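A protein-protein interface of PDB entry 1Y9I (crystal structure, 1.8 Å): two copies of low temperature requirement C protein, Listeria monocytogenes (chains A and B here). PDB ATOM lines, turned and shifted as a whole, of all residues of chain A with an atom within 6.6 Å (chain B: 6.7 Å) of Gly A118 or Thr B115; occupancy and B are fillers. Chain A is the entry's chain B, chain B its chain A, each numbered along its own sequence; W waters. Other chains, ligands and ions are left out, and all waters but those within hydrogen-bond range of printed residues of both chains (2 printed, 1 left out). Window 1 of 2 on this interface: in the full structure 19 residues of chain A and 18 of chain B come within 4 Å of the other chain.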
ATOM      1  N   GLU A  99      18.073   2.772 -13.321  1.00  0.00           N
ATOM      2  CA  GLU A  99      19.360   2.890 -14.012  1.00  0.00           C
ATOM      3  C   GLU A  99      20.369   1.878 -13.446  1.00  0.00           C
ATOM      4  O   GLU A  99      21.237   1.387 -14.163  1.00  0.00           O
ATOM      5  CB  GLU A  99      19.920   4.311 -13.885  1.00  0.00           C
ATOM      6  CG  GLU A  99      19.175   5.357 -14.730  1.00  0.00           C
ATOM      7  CD  GLU A  99      17.922   5.902 -14.062  1.00  0.00           C
ATOM      8  OE1 GLU A  99      17.582   5.445 -12.953  1.00  0.00           O
ATOM      9  OE2 GLU A  99      17.273   6.795 -14.649  1.00  0.00           O
ATOM     10  N   GLY A 113      30.255  -0.532 -23.060  1.00  0.00           N
ATOM     11  CA  GLY A 113      28.857  -0.387 -23.413  1.00  0.00           C
ATOM     12  C   GLY A 113      28.213   0.783 -22.679  1.00  0.00           C
ATOM     13  O   GLY A 113      27.120   1.216 -23.048  1.00  0.00           O
ATOM     14  N   PHE A 114      28.891   1.303 -21.653  1.00  0.00           N
ATOM     15  CA  PHE A 114      28.364   2.427 -20.862  1.00  0.00           C
ATOM     16  C   PHE A 114      27.934   3.614 -21.713  1.00  0.00           C
ATOM     17  O   PHE A 114      26.837   4.149 -21.543  1.00  0.00           O
ATOM     18  CB  PHE A 114      29.399   2.933 -19.840  1.00  0.00           C
ATOM     19  CG  PHE A 114      29.729   1.950 -18.747  1.00  0.00           C
ATOM     20  CD1 PHE A 114      28.982   0.788 -18.567  1.00  0.00           C
ATOM     21  CD2 PHE A 114      30.788   2.206 -17.880  1.00  0.00           C
ATOM     22  CE1 PHE A 114      29.288  -0.110 -17.537  1.00  0.00           C
ATOM     23  CE2 PHE A 114      31.102   1.316 -16.849  1.00  0.00           C
ATOM     24  CZ  PHE A 114      30.350   0.156 -16.680  1.00  0.00           C
ATOM     25  N   THR A 115      28.810   4.034 -22.618  1.00  0.00           N
ATOM     26  CA  THR A 115      28.528   5.172 -23.487  1.00  0.00           C
ATOM     27  C   THR A 115      27.240   5.042 -24.293  1.00  0.00           C
ATOM     28  O   THR A 115      26.382   5.931 -24.247  1.00  0.00           O
ATOM     29  CB  THR A 115      29.695   5.412 -24.467  1.00  0.00           C
ATOM     30  OG1 THR A 115      30.871   5.738 -23.727  1.00  0.00           O
ATOM     31  CG2 THR A 115      29.374   6.544 -25.413  1.00  0.00           C
ATOM     32  N   ASN A 116      27.109   3.946 -25.040  1.00  0.00           N
ATOM     33  CA  ASN A 116      25.918   3.734 -25.854  1.00  0.00           C
ATOM     34  C   ASN A 116      24.638   3.659 -25.033  1.00  0.00           C
ATOM     35  O   ASN A 116      23.576   4.082 -25.494  1.00  0.00           O
ATOM     36  CB  ASN A 116      26.060   2.474 -26.714  1.00  0.00           C
ATOM     37  CG  ASN A 116      26.854   2.732 -27.988  1.00  0.00           C
ATOM     38  OD1 ASN A 116      26.841   3.844 -28.521  1.00  0.00           O
ATOM     39  ND2 ASN A 116      27.532   1.703 -28.488  1.00  0.00           N
ATOM     40  N   TYR A 117      24.732   3.118 -23.822  1.00  0.00           N
ATOM     41  CA  TYR A 117      23.557   3.033 -22.967  1.00  0.00           C
ATOM     42  C   TYR A 117      23.074   4.439 -22.612  1.00  0.00           C
ATOM     43  O   TYR A 117      21.893   4.747 -22.753  1.00  0.00           O
ATOM     44  CB  TYR A 117      23.870   2.261 -21.682  1.00  0.00           C
ATOM     45  CG  TYR A 117      22.855   2.515 -20.584  1.00  0.00           C
ATOM     46  CD1 TYR A 117      21.493   2.270 -20.789  1.00  0.00           C
ATOM     47  CD2 TYR A 117      23.252   3.045 -19.358  1.00  0.00           C
ATOM     48  CE1 TYR A 117      20.547   2.557 -19.792  1.00  0.00           C
ATOM     49  CE2 TYR A 117      22.317   3.334 -18.357  1.00  0.00           C
ATOM     50  CZ  TYR A 117      20.971   3.091 -18.582  1.00  0.00           C
ATOM     51  OH  TYR A 117      20.056   3.407 -17.602  1.00  0.00           O
ATOM     52  N   GLY A 118      23.989   5.291 -22.153  1.00  0.00           N
ATOM     53  CA  GLY A 118      23.610   6.649 -21.789  1.00  0.00           C
ATOM     54  C   GLY A 118      23.145   7.454 -22.987  1.00  0.00           C
ATOM     55  O   GLY A 118      22.150   8.175 -22.925  1.00  0.00           O
ATOM     56  N   TYR A 119      23.862   7.322 -24.096  1.00  0.00           N
ATOM     57  CA  TYR A 119      23.503   8.057 -25.300  1.00  0.00           C
ATOM     58  C   TYR A 119      22.105   7.697 -25.799  1.00  0.00           C
ATOM     59  O   TYR A 119      21.277   8.575 -26.045  1.00  0.00           O
ATOM     60  CB  TYR A 119      24.530   7.785 -26.399  1.00  0.00           C
ATOM     61  CG  TYR A 119      24.211   8.490 -27.690  1.00  0.00           C
ATOM     62  CD1 TYR A 119      24.280   9.879 -27.781  1.00  0.00           C
ATOM     63  CD2 TYR A 119      23.810   7.772 -28.816  1.00  0.00           C
ATOM     64  CE1 TYR A 119      23.956  10.538 -28.958  1.00  0.00           C
ATOM     65  CE2 TYR A 119      23.480   8.424 -30.003  1.00  0.00           C
ATOM     66  CZ  TYR A 119      23.556   9.805 -30.064  1.00  0.00           C
ATOM     67  OH  TYR A 119      23.231  10.459 -31.228  1.00  0.00           O
ATOM     68  N   ILE A 120      21.833   6.403 -25.934  1.00  0.00           N
ATOM     69  CA  ILE A 120      20.537   5.974 -26.424  1.00  0.00           C
ATOM     70  C   ILE A 120      19.419   6.326 -25.443  1.00  0.00           C
ATOM     71  O   ILE A 120      18.305   6.642 -25.852  1.00  0.00           O
ATOM     72  CB  ILE A 120      20.534   4.448 -26.726  1.00  0.00           C
ATOM     73  CG1 ILE A 120      19.507   4.136 -27.814  1.00  0.00           C
ATOM     74  CG2 ILE A 120      20.243   3.651 -25.467  1.00  0.00           C
ATOM     75  CD1 ILE A 120      19.908   4.639 -29.184  1.00  0.00           C
ATOM     76  N   ASP A 121      19.713   6.268 -24.149  1.00  0.00           N
ATOM     77  CA  ASP A 121      18.708   6.599 -23.143  1.00  0.00           C
ATOM     78  C   ASP A 121      18.340   8.084 -23.182  1.00  0.00           C
ATOM     79  O   ASP A 121      17.222   8.458 -22.834  1.00  0.00           O
ATOM     80  CB  ASP A 121      19.204   6.248 -21.740  1.00  0.00           C
ATOM     81  CG  ASP A 121      18.149   6.503 -20.670  1.00  0.00           C
ATOM     82  OD1 ASP A 121      17.152   5.750 -20.626  1.00  0.00           O
ATOM     83  OD2 ASP A 121      18.312   7.460 -19.883  1.00  0.00           O
ATOM     84  N   LYS A 122      19.273   8.936 -23.598  1.00  0.00           N
ATOM     85  CA  LYS A 122      18.970  10.363 -23.654  1.00  0.00           C
ATOM     86  C   LYS A 122      18.274  10.747 -24.953  1.00  0.00           C
ATOM     87  O   LYS A 122      17.326  11.529 -24.940  1.00  0.00           O
ATOM     88  CB  LYS A 122      20.243  11.200 -23.472  1.00  0.00           C
ATOM     89  CG  LYS A 122      20.944  10.999 -22.132  1.00  0.00           C
ATOM     90  CD  LYS A 122      20.062  11.350 -20.933  1.00  0.00           C
ATOM     91  CE  LYS A 122      19.714  12.832 -20.881  1.00  0.00           C
ATOM     92  NZ  LYS A 122      18.978  13.178 -19.622  1.00  0.00           N
ATOM     93  N   VAL A 123      18.733  10.187 -26.069  1.00  0.00           N
ATOM     94  CA  VAL A 123      18.148  10.488 -27.373  1.00  0.00           C
ATOM     95  C   VAL A 123      16.782   9.822 -27.559  1.00  0.00           C
ATOM     96  O   VAL A 123      15.884  10.393 -28.179  1.00  0.00           O
ATOM     97  CB  VAL A 123      19.092  10.042 -28.505  1.00  0.00           C
ATOM     98  CG1 VAL A 123      18.493  10.392 -29.862  1.00  0.00           C
ATOM     99  CG2 VAL A 123      20.447  10.718 -28.337  1.00  0.00           C
ATOM    100  N   ASP A 145      14.984   1.733 -19.542  1.00  0.00           N
ATOM    101  CA  ASP A 145      16.419   1.553 -19.313  1.00  0.00           C
ATOM    102  C   ASP A 145      16.847   0.139 -19.691  1.00  0.00           C
ATOM    103  O   ASP A 145      17.943  -0.070 -20.216  1.00  0.00           O
ATOM    104  CB  ASP A 145      16.768   1.844 -17.849  1.00  0.00           C
ATOM    105  CG  ASP A 145      16.600   3.311 -17.492  1.00  0.00           C
ATOM    106  OD1 ASP A 145      17.450   4.136 -17.897  1.00  0.00           O
ATOM    107  OD2 ASP A 145      15.611   3.643 -16.812  1.00  0.00           O
ATOM    108  N   ALA A 152      22.635  -1.562 -25.882  1.00  0.00           N
ATOM    109  CA  ALA A 152      24.024  -1.212 -25.640  1.00  0.00           C
ATOM    110  C   ALA A 152      24.884  -2.466 -25.471  1.00  0.00           C
ATOM    111  O   ALA A 152      25.988  -2.539 -26.007  1.00  0.00           O
ATOM    112  CB  ALA A 152      24.136  -0.318 -24.407  1.00  0.00           C
ATOM    113  N   LEU B  35      24.125  19.846 -20.259  1.00  0.00           N
ATOM    114  CA  LEU B  35      23.340  18.714 -19.774  1.00  0.00           C
ATOM    115  C   LEU B  35      22.026  19.057 -19.077  1.00  0.00           C
ATOM    116  O   LEU B  35      21.059  18.297 -19.169  1.00  0.00           O
ATOM    117  CB  LEU B  35      24.170  17.893 -18.795  1.00  0.00           C
ATOM    118  CG  LEU B  35      25.390  17.149 -19.329  1.00  0.00           C
ATOM    119  CD1 LEU B  35      26.126  16.495 -18.167  1.00  0.00           C
ATOM    120  CD2 LEU B  35      24.944  16.102 -20.333  1.00  0.00           C
ATOM    121  N   VAL B 106      31.339   9.538 -11.388  1.00  0.00           N
ATOM    122  CA  VAL B 106      29.892   9.696 -11.521  1.00  0.00           C
ATOM    123  C   VAL B 106      29.170   9.193 -10.273  1.00  0.00           C
ATOM    124  O   VAL B 106      28.246   9.840  -9.758  1.00  0.00           O
ATOM    125  CB  VAL B 106      29.355   8.894 -12.724  1.00  0.00           C
ATOM    126  CG1 VAL B 106      27.833   9.022 -12.801  1.00  0.00           C
ATOM    127  CG2 VAL B 106      29.993   9.388 -14.007  1.00  0.00           C
ATOM    128  N   SER B 111      23.487   6.883  -9.339  1.00  0.00           N
ATOM    129  CA  SER B 111      23.137   6.356 -10.648  1.00  0.00           C
ATOM    130  C   SER B 111      22.401   7.312 -11.577  1.00  0.00           C
ATOM    131  O   SER B 111      22.393   7.103 -12.790  1.00  0.00           O
ATOM    132  CB  SER B 111      22.302   5.091 -10.476  1.00  0.00           C
ATOM    133  OG  SER B 111      21.156   5.366  -9.691  1.00  0.00           O
ATOM    134  N   ILE B 112      21.771   8.349 -11.035  1.00  0.00           N
ATOM    135  CA  ILE B 112      21.052   9.267 -11.914  1.00  0.00           C
ATOM    136  C   ILE B 112      21.995  10.049 -12.829  1.00  0.00           C
ATOM    137  O   ILE B 112      21.553  10.776 -13.717  1.00  0.00           O
ATOM    138  CB  ILE B 112      20.171  10.260 -11.136  1.00  0.00           C
ATOM    139  CG1 ILE B 112      21.026  11.201 -10.298  1.00  0.00           C
ATOM    140  CG2 ILE B 112      19.181   9.499 -10.264  1.00  0.00           C
ATOM    141  CD1 ILE B 112      20.246  12.407  -9.811  1.00  0.00           C
ATOM    142  N   GLY B 113      23.295   9.893 -12.616  1.00  0.00           N
ATOM    143  CA  GLY B 113      24.255  10.576 -13.465  1.00  0.00           C
ATOM    144  C   GLY B 113      24.757   9.677 -14.589  1.00  0.00           C
ATOM    145  O   GLY B 113      25.417  10.152 -15.522  1.00  0.00           O
ATOM    146  N   PHE B 114      24.425   8.389 -14.516  1.00  0.00           N
ATOM    147  CA  PHE B 114      24.855   7.396 -15.511  1.00  0.00           C
ATOM    148  C   PHE B 114      24.566   7.772 -16.965  1.00  0.00           C
ATOM    149  O   PHE B 114      25.467   7.776 -17.795  1.00  0.00           O
ATOM    150  CB  PHE B 114      24.203   6.024 -15.247  1.00  0.00           C
ATOM    151  CG  PHE B 114      24.717   5.303 -14.022  1.00  0.00           C
ATOM    152  CD1 PHE B 114      25.783   5.801 -13.273  1.00  0.00           C
ATOM    153  CD2 PHE B 114      24.131   4.102 -13.628  1.00  0.00           C
ATOM    154  CE1 PHE B 114      26.262   5.108 -12.150  1.00  0.00           C
ATOM    155  CE2 PHE B 114      24.600   3.402 -12.508  1.00  0.00           C
ATOM    156  CZ  PHE B 114      25.668   3.909 -11.769  1.00  0.00           C
ATOM    157  N   THR B 115      23.309   8.074 -17.283  1.00  0.00           N
ATOM    158  CA  THR B 115      22.972   8.404 -18.660  1.00  0.00           C
ATOM    159  C   THR B 115      23.649   9.672 -19.197  1.00  0.00           C
ATOM    160  O   THR B 115      24.051   9.709 -20.359  1.00  0.00           O
ATOM    161  CB  THR B 115      21.430   8.465 -18.856  1.00  0.00           C
ATOM    162  OG1 THR B 115      20.841   9.298 -17.854  1.00  0.00           O
ATOM    163  CG2 THR B 115      20.835   7.063 -18.743  1.00  0.00           C
ATOM    164  N   ASN B 116      23.809  10.695 -18.363  1.00  0.00           N
ATOM    165  CA  ASN B 116      24.466  11.909 -18.832  1.00  0.00           C
ATOM    166  C   ASN B 116      25.934  11.652 -19.135  1.00  0.00           C
ATOM    167  O   ASN B 116      26.519  12.276 -20.022  1.00  0.00           O
ATOM    168  CB  ASN B 116      24.334  13.043 -17.810  1.00  0.00           C
ATOM    169  CG  ASN B 116      23.048  13.833 -17.992  1.00  0.00           C
ATOM    170  OD1 ASN B 116      22.437  13.790 -19.058  1.00  0.00           O
ATOM    171  ND2 ASN B 116      22.644  14.568 -16.963  1.00  0.00           N
ATOM    172  N   TYR B 117      26.529  10.730 -18.389  1.00  0.00           N
ATOM    173  CA  TYR B 117      27.928  10.367 -18.592  1.00  0.00           C
ATOM    174  C   TYR B 117      28.092   9.752 -19.987  1.00  0.00           C
ATOM    175  O   TYR B 117      28.957  10.171 -20.764  1.00  0.00           O
ATOM    176  CB  TYR B 117      28.341   9.376 -17.502  1.00  0.00           C
ATOM    177  CG  TYR B 117      29.695   8.719 -17.672  1.00  0.00           C
ATOM    178  CD1 TYR B 117      30.850   9.478 -17.849  1.00  0.00           C
ATOM    179  CD2 TYR B 117      29.826   7.333 -17.563  1.00  0.00           C
ATOM    180  CE1 TYR B 117      32.108   8.873 -17.900  1.00  0.00           C
ATOM    181  CE2 TYR B 117      31.071   6.717 -17.614  1.00  0.00           C
ATOM    182  CZ  TYR B 117      32.210   7.492 -17.778  1.00  0.00           C
ATOM    183  OH  TYR B 117      33.442   6.882 -17.790  1.00  0.00           O
ATOM    184  N   GLY B 118      27.246   8.776 -20.309  1.00  0.00           N
ATOM    185  CA  GLY B 118      27.326   8.138 -21.609  1.00  0.00           C
ATOM    186  C   GLY B 118      26.991   9.084 -22.745  1.00  0.00           C
ATOM    187  O   GLY B 118      27.698   9.141 -23.747  1.00  0.00           O
ATOM    188  N   TYR B 119      25.907   9.837 -22.579  1.00  0.00           N
ATOM    189  CA  TYR B 119      25.451  10.777 -23.593  1.00  0.00           C
ATOM    190  C   TYR B 119      26.493  11.828 -23.954  1.00  0.00           C
ATOM    191  O   TYR B 119      26.759  12.074 -25.131  1.00  0.00           O
ATOM    192  CB  TYR B 119      24.173  11.470 -23.106  1.00  0.00           C
ATOM    193  CG  TYR B 119      23.676  12.578 -24.013  1.00  0.00           C
ATOM    194  CD1 TYR B 119      23.229  12.303 -25.305  1.00  0.00           C
ATOM    195  CD2 TYR B 119      23.645  13.901 -23.572  1.00  0.00           C
ATOM    196  CE1 TYR B 119      22.760  13.316 -26.136  1.00  0.00           C
ATOM    197  CE2 TYR B 119      23.178  14.924 -24.396  1.00  0.00           C
ATOM    198  CZ  TYR B 119      22.737  14.622 -25.673  1.00  0.00           C
ATOM    199  OH  TYR B 119      22.268  15.622 -26.488  1.00  0.00           O
ATOM    200  N   ILE B 120      27.096  12.448 -22.943  1.00  0.00           N
ATOM    201  CA  ILE B 120      28.072  13.491 -23.209  1.00  0.00           C
ATOM    202  C   ILE B 120      29.335  12.926 -23.849  1.00  0.00           C
ATOM    203  O   ILE B 120      29.997  13.604 -24.635  1.00  0.00           O
ATOM    204  CB  ILE B 120      28.408  14.287 -21.922  1.00  0.00           C
ATOM    205  CG1 ILE B 120      28.936  15.674 -22.312  1.00  0.00           C
ATOM    206  CG2 ILE B 120      29.430  13.530 -21.072  1.00  0.00           C
ATOM    207  CD1 ILE B 120      28.934  16.685 -21.185  1.00  0.00           C
ATOM    208  N   ALA B 152      28.856  15.102 -15.459  1.00  0.00           N
ATOM    209  CA  ALA B 152      27.679  14.306 -15.140  1.00  0.00           C
ATOM    210  C   ALA B 152      27.423  14.273 -13.636  1.00  0.00           C
ATOM    211  O   ALA B 152      26.278  14.332 -13.193  1.00  0.00           O
ATOM    212  CB  ALA B 152      27.845  12.884 -15.676  1.00  0.00           C
HETATM  213  O   HOH W   1      19.714  12.715 -16.682  1.00  0.00           O
HETATM  214  O   HOH W   2      21.199  15.649 -20.524  1.00  0.00           O
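The side-chain carboxylate of Asp A145 is in hydrogen-bond range of the side-chain hydroxyl of Tyr A117 (2.7 Å).
Among the printed residues, merely in contact across the chains: Asp A121 with Thr B115 (2.8 Å), Lys A122 with Tyr B119 (3.4 Å), Gly A118 with Thr B115 (3.4 Å), Lys A122 with Asn B116 (3.4 Å), Thr A115 with Gly B118 (3.5 Å), Tyr A119 with Tyr B119 (3.6 Å), Gly A118 with Tyr B119 (3.7 Å), Lys A122 with Thr B115 (3.8 Å), Tyr A119 with Gly B118 (3.8 Å), Glu A99 with Ser B111 (3.9 Å) and Tyr A117 with Thr B115 (3.9 Å).
Printed residues of chain B within 4 Å of Gly A118: Thr B115 (3.4 Å) and Tyr B119 (3.7 Å).
Of chain A, only Tyr A117, Gly A118, Asp A121 and Lys A122 come within 4 Å of Thr B115.
Printed residues of chain B within 4 Å of Tyr A119: Gly B118 and Tyr B119.
Of the printed residues of chain B, Thr A115 touches Gly B118.
Of the printed residues of chain A, Gly B118 touches Thr A115 (3.5 Å) and Tyr A119 (3.8 Å).
Val A123 touches none of the printed residues of chain B.
The nearest printed residue of chain B that does not touch Gly A118 is Gly B118 (4.01 Å).
The nearest residue of chain A that does not touch Thr B115 is Tyr A119 (4.4 Å).
Hydrophobic or aromatic side chains of chain A that line the printed part of chain B: Tyr A117 and Tyr A119.
Among the printed residues, 11 pairs touch across the chains.
Among the printed residues, no Asp or Glu carboxylate lies within 4 Å of a Lys or Arg side-chain nitrogen of the other chain.
Thr A115 touches Gly B118, and with the chains exchanged Gly A118 touches Thr B115.
Tyr A117 touches Thr B115, but with the chains exchanged Thr A115 does not touch Tyr B117 (5.7 Å).
Gly A118 touches Tyr B119, and with the chains exchanged Tyr A119 touches Gly B118.
Tyr B119 touches its own counterpart, Tyr A119.
Positions printed for both chains: 113, 114, 115, 116, 117, 118, 119, 120 and 152.
Of the 11 pairs that touch across the chains among the printed residues, 5 have their exchanged pair printed and touching as well.
Water W2 lies within hydrogen-bond range of the side-chain amide oxygen (OD1) of Asn B116 (2.7 Å), the backbone carbonyl oxygen (O) of Leu B35 (3.0 Å) and the side-chain amino group (NZ) of Lys A122 (3.4 Å).
Water W1 lies within hydrogen-bond range of NZ of Lys A122 (3.1 Å) and ND2 of Asn B116 (3.5 Å).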
